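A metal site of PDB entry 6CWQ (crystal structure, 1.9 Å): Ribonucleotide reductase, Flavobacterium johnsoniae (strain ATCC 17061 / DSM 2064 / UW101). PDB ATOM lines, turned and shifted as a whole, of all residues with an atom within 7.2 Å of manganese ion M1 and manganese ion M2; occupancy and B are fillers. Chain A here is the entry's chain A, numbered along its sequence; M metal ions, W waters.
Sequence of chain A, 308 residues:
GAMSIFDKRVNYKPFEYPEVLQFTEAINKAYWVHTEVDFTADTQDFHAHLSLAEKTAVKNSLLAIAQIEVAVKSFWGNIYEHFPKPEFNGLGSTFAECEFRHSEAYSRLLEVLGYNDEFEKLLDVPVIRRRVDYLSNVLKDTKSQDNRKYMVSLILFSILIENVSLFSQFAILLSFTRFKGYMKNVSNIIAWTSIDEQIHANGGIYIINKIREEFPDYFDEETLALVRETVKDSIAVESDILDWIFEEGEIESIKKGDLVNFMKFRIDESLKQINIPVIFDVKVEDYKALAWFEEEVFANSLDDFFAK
Manganese ion M2 is bound by OE2 of Glu 197 (1.9 Å), OE1 of Glu 69 (2.3 Å), ND1 of His 102 (2.3 Å), OE2 of Glu 69 (2.4 Å) and OE1 of Glu 99 (2.4 Å). Manganese ion M2 has five donor atoms within binding distance. Slightly farther from manganese ion M2 lies water W2 (2.9 Å).
Within 4 Å of manganese ion M1: Glu 99, Glu 162, Glu 197 and His 200. The nearest printed residue that does not touch manganese ion M1 is Trp 76 (4.5 Å).
NE2 of His 102 is in hydrogen-bond range of SG of Cys 98. NE1 of Trp 76 sits close to OE1 of Glu 162 (2.8 Å). O of Glu 99 lies within hydrogen-bond range of OG of Ser 103 (3.4 Å). NE2 of His 200 sits at hydrogen-bond distance from SG of Cys 98, 3.5 Å away. The side-chain amino group of Lys 73 is in hydrogen-bond range of the backbone carbonyl oxygen of Glu 69, 2.9 Å away. A ring nitrogen (NE2) of His 102 sits at hydrogen-bond distance from the side-chain carboxylate (OD2) of Asp 196 (2.9 Å). O of Phe 157 sits at hydrogen-bond distance from N of Glu 162 (3.1 Å). The backbone carbonyl oxygen of Glu 99 is in hydrogen-bond range of the side-chain amino group of Lys 73.
Of the 22 residues printed, 4 come within 4 Å of manganese ion M2. The nearest printed residue that does not touch manganese ion M2 is Lys 73 (4.1 Å).
Manganese ion M1 is bound by OE1 of Glu 197 (2.1 Å). OE2 of Glu 99 is bound to manganese ion M1 (2.3 Å). Manganese ion M1 is bound by ND1 of His 200 (2.4 Å). Manganese ion M1 is bound by water W1, 2.4 Å away. The side-chain carboxylate (OE1) of Glu 162 binds manganese ion M1, at 2.5 Å. Slightly farther from manganese ion M1 lies water W2 (2.8 Å). Slightly farther from manganese ion M1 lies the side-chain carboxylate (OE2) of Glu 162 (2.9 Å).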
ATOM      1  N   ILE A  68     -24.184  18.708  27.900  1.00  0.00           N
ATOM      2  CA  ILE A  68     -23.082  19.526  27.379  1.00  0.00           C
ATOM      3  C   ILE A  68     -22.362  18.870  26.188  1.00  0.00           C
ATOM      4  O   ILE A  68     -22.049  19.551  25.206  1.00  0.00           O
ATOM      5  CB  ILE A  68     -22.096  19.902  28.509  1.00  0.00           C
ATOM      6  CG1 ILE A  68     -22.741  20.954  29.419  1.00  0.00           C
ATOM      7  CG2 ILE A  68     -20.781  20.431  27.957  1.00  0.00           C
ATOM      8  CD1 ILE A  68     -22.020  21.179  30.717  1.00  0.00           C
ATOM      9  N   GLU A  69     -22.121  17.561  26.261  1.00  0.00           N
ATOM     10  CA  GLU A  69     -21.250  16.900  25.297  1.00  0.00           C
ATOM     11  C   GLU A  69     -21.930  16.472  23.996  1.00  0.00           C
ATOM     12  O   GLU A  69     -21.271  16.409  22.962  1.00  0.00           O
ATOM     13  CB  GLU A  69     -20.568  15.669  25.922  1.00  0.00           C
ATOM     14  CG  GLU A  69     -19.586  15.992  27.045  1.00  0.00           C
ATOM     15  CD  GLU A  69     -18.263  16.536  26.551  1.00  0.00           C
ATOM     16  OE1 GLU A  69     -18.176  17.052  25.433  1.00  0.00           O
ATOM     17  OE2 GLU A  69     -17.278  16.437  27.300  1.00  0.00           O
ATOM     18  N   LYS A  73     -20.586  21.858  19.118  1.00  0.00           N
ATOM     19  CA  LYS A  73     -19.812  22.801  19.931  1.00  0.00           C
ATOM     20  C   LYS A  73     -18.814  23.503  19.028  1.00  0.00           C
ATOM     21  O   LYS A  73     -17.795  22.919  18.667  1.00  0.00           O
ATOM     22  CB  LYS A  73     -19.100  22.056  21.072  1.00  0.00           C
ATOM     23  CG  LYS A  73     -20.009  21.445  22.125  1.00  0.00           C
ATOM     24  CD  LYS A  73     -19.371  20.267  22.857  1.00  0.00           C
ATOM     25  CE  LYS A  73     -19.475  18.970  22.056  1.00  0.00           C
ATOM     26  NZ  LYS A  73     -18.746  17.792  22.639  1.00  0.00           N
ATOM     27  N   TRP A  76     -14.211  26.262  19.950  1.00  0.00           N
ATOM     28  CA  TRP A  76     -12.785  26.019  19.669  1.00  0.00           C
ATOM     29  C   TRP A  76     -12.464  26.094  18.181  1.00  0.00           C
ATOM     30  O   TRP A  76     -11.465  26.704  17.792  1.00  0.00           O
ATOM     31  CB  TRP A  76     -12.342  24.674  20.236  1.00  0.00           C
ATOM     32  CG  TRP A  76     -12.169  24.709  21.712  1.00  0.00           C
ATOM     33  CD1 TRP A  76     -12.861  23.990  22.642  1.00  0.00           C
ATOM     34  CD2 TRP A  76     -11.243  25.523  22.441  1.00  0.00           C
ATOM     35  NE1 TRP A  76     -12.409  24.292  23.902  1.00  0.00           N
ATOM     36  CE2 TRP A  76     -11.427  25.245  23.811  1.00  0.00           C
ATOM     37  CE3 TRP A  76     -10.263  26.451  22.059  1.00  0.00           C
ATOM     38  CZ2 TRP A  76     -10.662  25.848  24.809  1.00  0.00           C
ATOM     39  CZ3 TRP A  76      -9.513  27.061  23.053  1.00  0.00           C
ATOM     40  CH2 TRP A  76      -9.718  26.762  24.414  1.00  0.00           C
ATOM     41  N   PHE A  95      -8.764  20.853  19.167  1.00  0.00           N
ATOM     42  CA  PHE A  95      -9.793  20.791  20.217  1.00  0.00           C
ATOM     43  C   PHE A  95     -11.197  20.572  19.641  1.00  0.00           C
ATOM     44  O   PHE A  95     -12.020  19.882  20.247  1.00  0.00           O
ATOM     45  CB  PHE A  95      -9.767  22.083  21.065  1.00  0.00           C
ATOM     46  CG  PHE A  95      -8.592  22.195  22.009  1.00  0.00           C
ATOM     47  CD1 PHE A  95      -7.552  21.269  22.020  1.00  0.00           C
ATOM     48  CD2 PHE A  95      -8.520  23.269  22.883  1.00  0.00           C
ATOM     49  CE1 PHE A  95      -6.490  21.401  22.895  1.00  0.00           C
ATOM     50  CE2 PHE A  95      -7.466  23.412  23.759  1.00  0.00           C
ATOM     51  CZ  PHE A  95      -6.453  22.476  23.779  1.00  0.00           C
ATOM     52  N   CYS A  98     -11.713  16.911  18.863  1.00  0.00           N
ATOM     53  CA  CYS A  98     -11.911  16.246  20.131  1.00  0.00           C
ATOM     54  C   CYS A  98     -13.393  16.234  20.552  1.00  0.00           C
ATOM     55  O   CYS A  98     -13.901  15.221  21.034  1.00  0.00           O
ATOM     56  CB  CYS A  98     -11.057  16.951  21.186  1.00  0.00           C
ATOM     57  SG  CYS A  98     -10.983  16.083  22.736  1.00  0.00           S
ATOM     58  N   GLU A  99     -14.058  17.374  20.368  1.00  0.00           N
ATOM     59  CA  GLU A  99     -15.457  17.502  20.777  1.00  0.00           C
ATOM     60  C   GLU A  99     -16.409  16.564  20.015  1.00  0.00           C
ATOM     61  O   GLU A  99     -17.449  16.174  20.543  1.00  0.00           O
ATOM     62  CB  GLU A  99     -15.911  18.954  20.681  1.00  0.00           C
ATOM     63  CG  GLU A  99     -15.311  19.873  21.755  1.00  0.00           C
ATOM     64  CD  GLU A  99     -15.442  19.320  23.171  1.00  0.00           C
ATOM     65  OE1 GLU A  99     -16.438  18.634  23.501  1.00  0.00           O
ATOM     66  OE2 GLU A  99     -14.519  19.571  23.987  1.00  0.00           O
ATOM     67  N   PHE A 100     -16.053  16.227  18.774  1.00  0.00           N
ATOM     68  CA  PHE A 100     -16.867  15.293  18.020  1.00  0.00           C
ATOM     69  C   PHE A 100     -16.617  13.865  18.512  1.00  0.00           C
ATOM     70  O   PHE A 100     -17.541  13.062  18.577  1.00  0.00           O
ATOM     71  CB  PHE A 100     -16.606  15.389  16.524  1.00  0.00           C
ATOM     72  CG  PHE A 100     -17.510  14.534  15.692  1.00  0.00           C
ATOM     73  CD1 PHE A 100     -18.883  14.757  15.713  1.00  0.00           C
ATOM     74  CD2 PHE A 100     -17.001  13.533  14.891  1.00  0.00           C
ATOM     75  CE1 PHE A 100     -19.729  13.973  14.954  1.00  0.00           C
ATOM     76  CE2 PHE A 100     -17.850  12.749  14.115  1.00  0.00           C
ATOM     77  CZ  PHE A 100     -19.214  12.969  14.146  1.00  0.00           C
ATOM     78  N   HIS A 102     -15.997  13.228  21.574  1.00  0.00           N
ATOM     79  CA  HIS A 102     -16.795  13.238  22.799  1.00  0.00           C
ATOM     80  C   HIS A 102     -18.292  13.087  22.566  1.00  0.00           C
ATOM     81  O   HIS A 102     -18.948  12.287  23.238  1.00  0.00           O
ATOM     82  CB  HIS A 102     -16.562  14.510  23.585  1.00  0.00           C
ATOM     83  CG  HIS A 102     -15.173  14.639  24.122  1.00  0.00           C
ATOM     84  ND1 HIS A 102     -14.751  15.749  24.817  1.00  0.00           N
ATOM     85  CD2 HIS A 102     -14.120  13.805  24.067  1.00  0.00           C
ATOM     86  CE1 HIS A 102     -13.490  15.596  25.166  1.00  0.00           C
ATOM     87  NE2 HIS A 102     -13.086  14.418  24.724  1.00  0.00           N
ATOM     88  N   SER A 103     -18.845  13.862  21.628  1.00  0.00           N
ATOM     89  CA  SER A 103     -20.282  13.789  21.352  1.00  0.00           C
ATOM     90  C   SER A 103     -20.669  12.378  20.904  1.00  0.00           C
ATOM     91  O   SER A 103     -21.711  11.855  21.325  1.00  0.00           O
ATOM     92  CB  SER A 103     -20.723  14.850  20.324  1.00  0.00           C
ATOM     93  OG  SER A 103     -20.139  14.674  19.049  1.00  0.00           O
ATOM     94  N   TYR A 106     -20.590   9.994  24.088  1.00  0.00           N
ATOM     95  CA  TYR A 106     -21.746  10.105  24.991  1.00  0.00           C
ATOM     96  C   TYR A 106     -23.061   9.749  24.334  1.00  0.00           C
ATOM     97  O   TYR A 106     -23.949   9.221  25.000  1.00  0.00           O
ATOM     98  CB  TYR A 106     -21.755  11.462  25.728  1.00  0.00           C
ATOM     99  CG  TYR A 106     -20.588  11.468  26.678  1.00  0.00           C
ATOM    100  CD1 TYR A 106     -20.657  10.775  27.890  1.00  0.00           C
ATOM    101  CD2 TYR A 106     -19.388  12.051  26.327  1.00  0.00           C
ATOM    102  CE1 TYR A 106     -19.565  10.716  28.746  1.00  0.00           C
ATOM    103  CE2 TYR A 106     -18.284  11.986  27.168  1.00  0.00           C
ATOM    104  CZ  TYR A 106     -18.377  11.320  28.373  1.00  0.00           C
ATOM    105  OH  TYR A 106     -17.284  11.259  29.188  1.00  0.00           O
ATOM    106  N   PHE A 157     -15.930  30.360  29.533  1.00  0.00           N
ATOM    107  CA  PHE A 157     -15.897  29.094  28.798  1.00  0.00           C
ATOM    108  C   PHE A 157     -14.854  28.142  29.405  1.00  0.00           C
ATOM    109  O   PHE A 157     -15.145  26.975  29.658  1.00  0.00           O
ATOM    110  CB  PHE A 157     -15.621  29.334  27.314  1.00  0.00           C
ATOM    111  CG  PHE A 157     -15.695  28.105  26.462  1.00  0.00           C
ATOM    112  CD1 PHE A 157     -16.904  27.704  25.912  1.00  0.00           C
ATOM    113  CD2 PHE A 157     -14.575  27.336  26.217  1.00  0.00           C
ATOM    114  CE1 PHE A 157     -16.986  26.555  25.127  1.00  0.00           C
ATOM    115  CE2 PHE A 157     -14.648  26.199  25.449  1.00  0.00           C
ATOM    116  CZ  PHE A 157     -15.850  25.803  24.903  1.00  0.00           C
ATOM    117  N   ILE A 161     -17.359  25.816  31.413  1.00  0.00           N
ATOM    118  CA  ILE A 161     -17.714  24.774  30.439  1.00  0.00           C
ATOM    119  C   ILE A 161     -16.666  23.657  30.382  1.00  0.00           C
ATOM    120  O   ILE A 161     -17.029  22.485  30.267  1.00  0.00           O
ATOM    121  CB  ILE A 161     -17.899  25.318  29.014  1.00  0.00           C
ATOM    122  CG1 ILE A 161     -18.897  26.489  28.958  1.00  0.00           C
ATOM    123  CG2 ILE A 161     -18.363  24.220  28.056  1.00  0.00           C
ATOM    124  CD1 ILE A 161     -20.262  26.166  29.503  1.00  0.00           C
ATOM    125  N   GLU A 162     -15.382  24.012  30.429  1.00  0.00           N
ATOM    126  CA  GLU A 162     -14.298  23.038  30.287  1.00  0.00           C
ATOM    127  C   GLU A 162     -13.776  22.454  31.605  1.00  0.00           C
ATOM    128  O   GLU A 162     -13.350  21.304  31.635  1.00  0.00           O
ATOM    129  CB  GLU A 162     -13.112  23.658  29.540  1.00  0.00           C
ATOM    130  CG  GLU A 162     -13.452  24.293  28.217  1.00  0.00           C
ATOM    131  CD  GLU A 162     -14.018  23.313  27.206  1.00  0.00           C
ATOM    132  OE1 GLU A 162     -13.340  23.039  26.213  1.00  0.00           O
ATOM    133  OE2 GLU A 162     -15.138  22.815  27.412  1.00  0.00           O
ATOM    134  N   LEU A 166     -18.722  19.884  34.090  1.00  0.00           N
ATOM    135  CA  LEU A 166     -18.784  18.437  33.871  1.00  0.00           C
ATOM    136  C   LEU A 166     -18.160  17.617  35.013  1.00  0.00           C
ATOM    137  O   LEU A 166     -18.513  16.452  35.194  1.00  0.00           O
ATOM    138  CB  LEU A 166     -18.046  18.074  32.586  1.00  0.00           C
ATOM    139  CG  LEU A 166     -18.615  18.618  31.274  1.00  0.00           C
ATOM    140  CD1 LEU A 166     -17.595  18.504  30.147  1.00  0.00           C
ATOM    141  CD2 LEU A 166     -19.881  17.870  30.910  1.00  0.00           C
ATOM    142  N   PHE A 170     -18.288  13.576  36.197  1.00  0.00           N
ATOM    143  CA  PHE A 170     -17.154  12.676  35.989  1.00  0.00           C
ATOM    144  C   PHE A 170     -16.784  11.961  37.295  1.00  0.00           C
ATOM    145  O   PHE A 170     -16.653  10.729  37.329  1.00  0.00           O
ATOM    146  CB  PHE A 170     -15.920  13.429  35.465  1.00  0.00           C
ATOM    147  CG  PHE A 170     -16.073  14.015  34.076  1.00  0.00           C
ATOM    148  CD1 PHE A 170     -17.012  13.543  33.172  1.00  0.00           C
ATOM    149  CD2 PHE A 170     -15.201  15.018  33.671  1.00  0.00           C
ATOM    150  CE1 PHE A 170     -17.092  14.077  31.906  1.00  0.00           C
ATOM    151  CE2 PHE A 170     -15.293  15.565  32.389  1.00  0.00           C
ATOM    152  CZ  PHE A 170     -16.233  15.088  31.514  1.00  0.00           C
ATOM    153  N   THR A 193     -12.213  11.384  28.698  1.00  0.00           N
ATOM    154  CA  THR A 193     -12.864  12.676  28.519  1.00  0.00           C
ATOM    155  C   THR A 193     -12.308  13.713  29.491  1.00  0.00           C
ATOM    156  O   THR A 193     -12.039  14.850  29.089  1.00  0.00           O
ATOM    157  CB  THR A 193     -14.392  12.584  28.707  1.00  0.00           C
ATOM    158  OG1 THR A 193     -14.926  11.574  27.843  1.00  0.00           O
ATOM    159  CG2 THR A 193     -15.049  13.916  28.372  1.00  0.00           C
ATOM    160  N   ASP A 196      -8.917  15.029  28.312  1.00  0.00           N
ATOM    161  CA  ASP A 196      -9.125  15.986  27.217  1.00  0.00           C
ATOM    162  C   ASP A 196      -9.636  17.324  27.724  1.00  0.00           C
ATOM    163  O   ASP A 196      -9.122  18.364  27.334  1.00  0.00           O
ATOM    164  CB  ASP A 196     -10.104  15.445  26.166  1.00  0.00           C
ATOM    165  CG  ASP A 196      -9.534  14.289  25.372  1.00  0.00           C
ATOM    166  OD1 ASP A 196      -8.302  14.094  25.338  1.00  0.00           O
ATOM    167  OD2 ASP A 196     -10.359  13.551  24.768  1.00  0.00           O
ATOM    168  N   GLU A 197     -10.653  17.300  28.591  1.00  0.00           N
ATOM    169  CA  GLU A 197     -11.266  18.535  29.043  1.00  0.00           C
ATOM    170  C   GLU A 197     -10.289  19.375  29.835  1.00  0.00           C
ATOM    171  O   GLU A 197     -10.301  20.608  29.735  1.00  0.00           O
ATOM    172  CB  GLU A 197     -12.505  18.282  29.914  1.00  0.00           C
ATOM    173  CG  GLU A 197     -13.666  17.625  29.206  1.00  0.00           C
ATOM    174  CD  GLU A 197     -14.115  18.351  27.953  1.00  0.00           C
ATOM    175  OE1 GLU A 197     -13.759  19.529  27.754  1.00  0.00           O
ATOM    176  OE2 GLU A 197     -14.839  17.725  27.165  1.00  0.00           O
ATOM    177  N   GLN A 198      -9.445  18.716  30.617  1.00  0.00           N
ATOM    178  CA  GLN A 198      -8.427  19.416  31.388  1.00  0.00           C
ATOM    179  C   GLN A 198      -7.436  20.130  30.487  1.00  0.00           C
ATOM    180  O   GLN A 198      -7.033  21.260  30.748  1.00  0.00           O
ATOM    181  CB  GLN A 198      -7.690  18.456  32.329  1.00  0.00           C
ATOM    182  CG  GLN A 198      -6.805  19.180  33.315  1.00  0.00           C
ATOM    183  CD  GLN A 198      -7.616  20.121  34.174  1.00  0.00           C
ATOM    184  OE1 GLN A 198      -8.493  19.687  34.904  1.00  0.00           O
ATOM    185  NE2 GLN A 198      -7.343  21.419  34.084  1.00  0.00           N
ATOM    186  N   HIS A 200      -8.194  21.154  27.475  1.00  0.00           N
ATOM    187  CA  HIS A 200      -8.952  22.285  26.919  1.00  0.00           C
ATOM    188  C   HIS A 200      -8.924  23.480  27.877  1.00  0.00           C
ATOM    189  O   HIS A 200      -8.656  24.593  27.457  1.00  0.00           O
ATOM    190  CB  HIS A 200     -10.404  21.923  26.577  1.00  0.00           C
ATOM    191  CG  HIS A 200     -10.525  20.833  25.565  1.00  0.00           C
ATOM    192  ND1 HIS A 200     -11.717  20.219  25.272  1.00  0.00           N
ATOM    193  CD2 HIS A 200      -9.590  20.217  24.796  1.00  0.00           C
ATOM    194  CE1 HIS A 200     -11.531  19.285  24.360  1.00  0.00           C
ATOM    195  NE2 HIS A 200     -10.244  19.259  24.057  1.00  0.00           N
ATOM    196  N   ALA A 201      -9.220  23.235  29.142  1.00  0.00           N
ATOM    197  CA  ALA A 201      -9.185  24.274  30.173  1.00  0.00           C
ATOM    198  C   ALA A 201      -7.813  24.927  30.263  1.00  0.00           C
ATOM    199  O   ALA A 201      -7.710  26.160  30.297  1.00  0.00           O
ATOM    200  CB  ALA A 201      -9.576  23.695  31.525  1.00  0.00           C
HETATM  201 MN    MN M   1     -13.943  20.593  25.944  1.00  0.00          MN
HETATM  202 MN    MN M   2     -15.946  17.564  25.625  1.00  0.00          MN
HETATM  203  O   HOH W   1     -15.444  21.998  24.696  1.00  0.00           O
HETATM  204  O   HOH W   2     -16.584  20.145  26.764  1.00  0.00           O
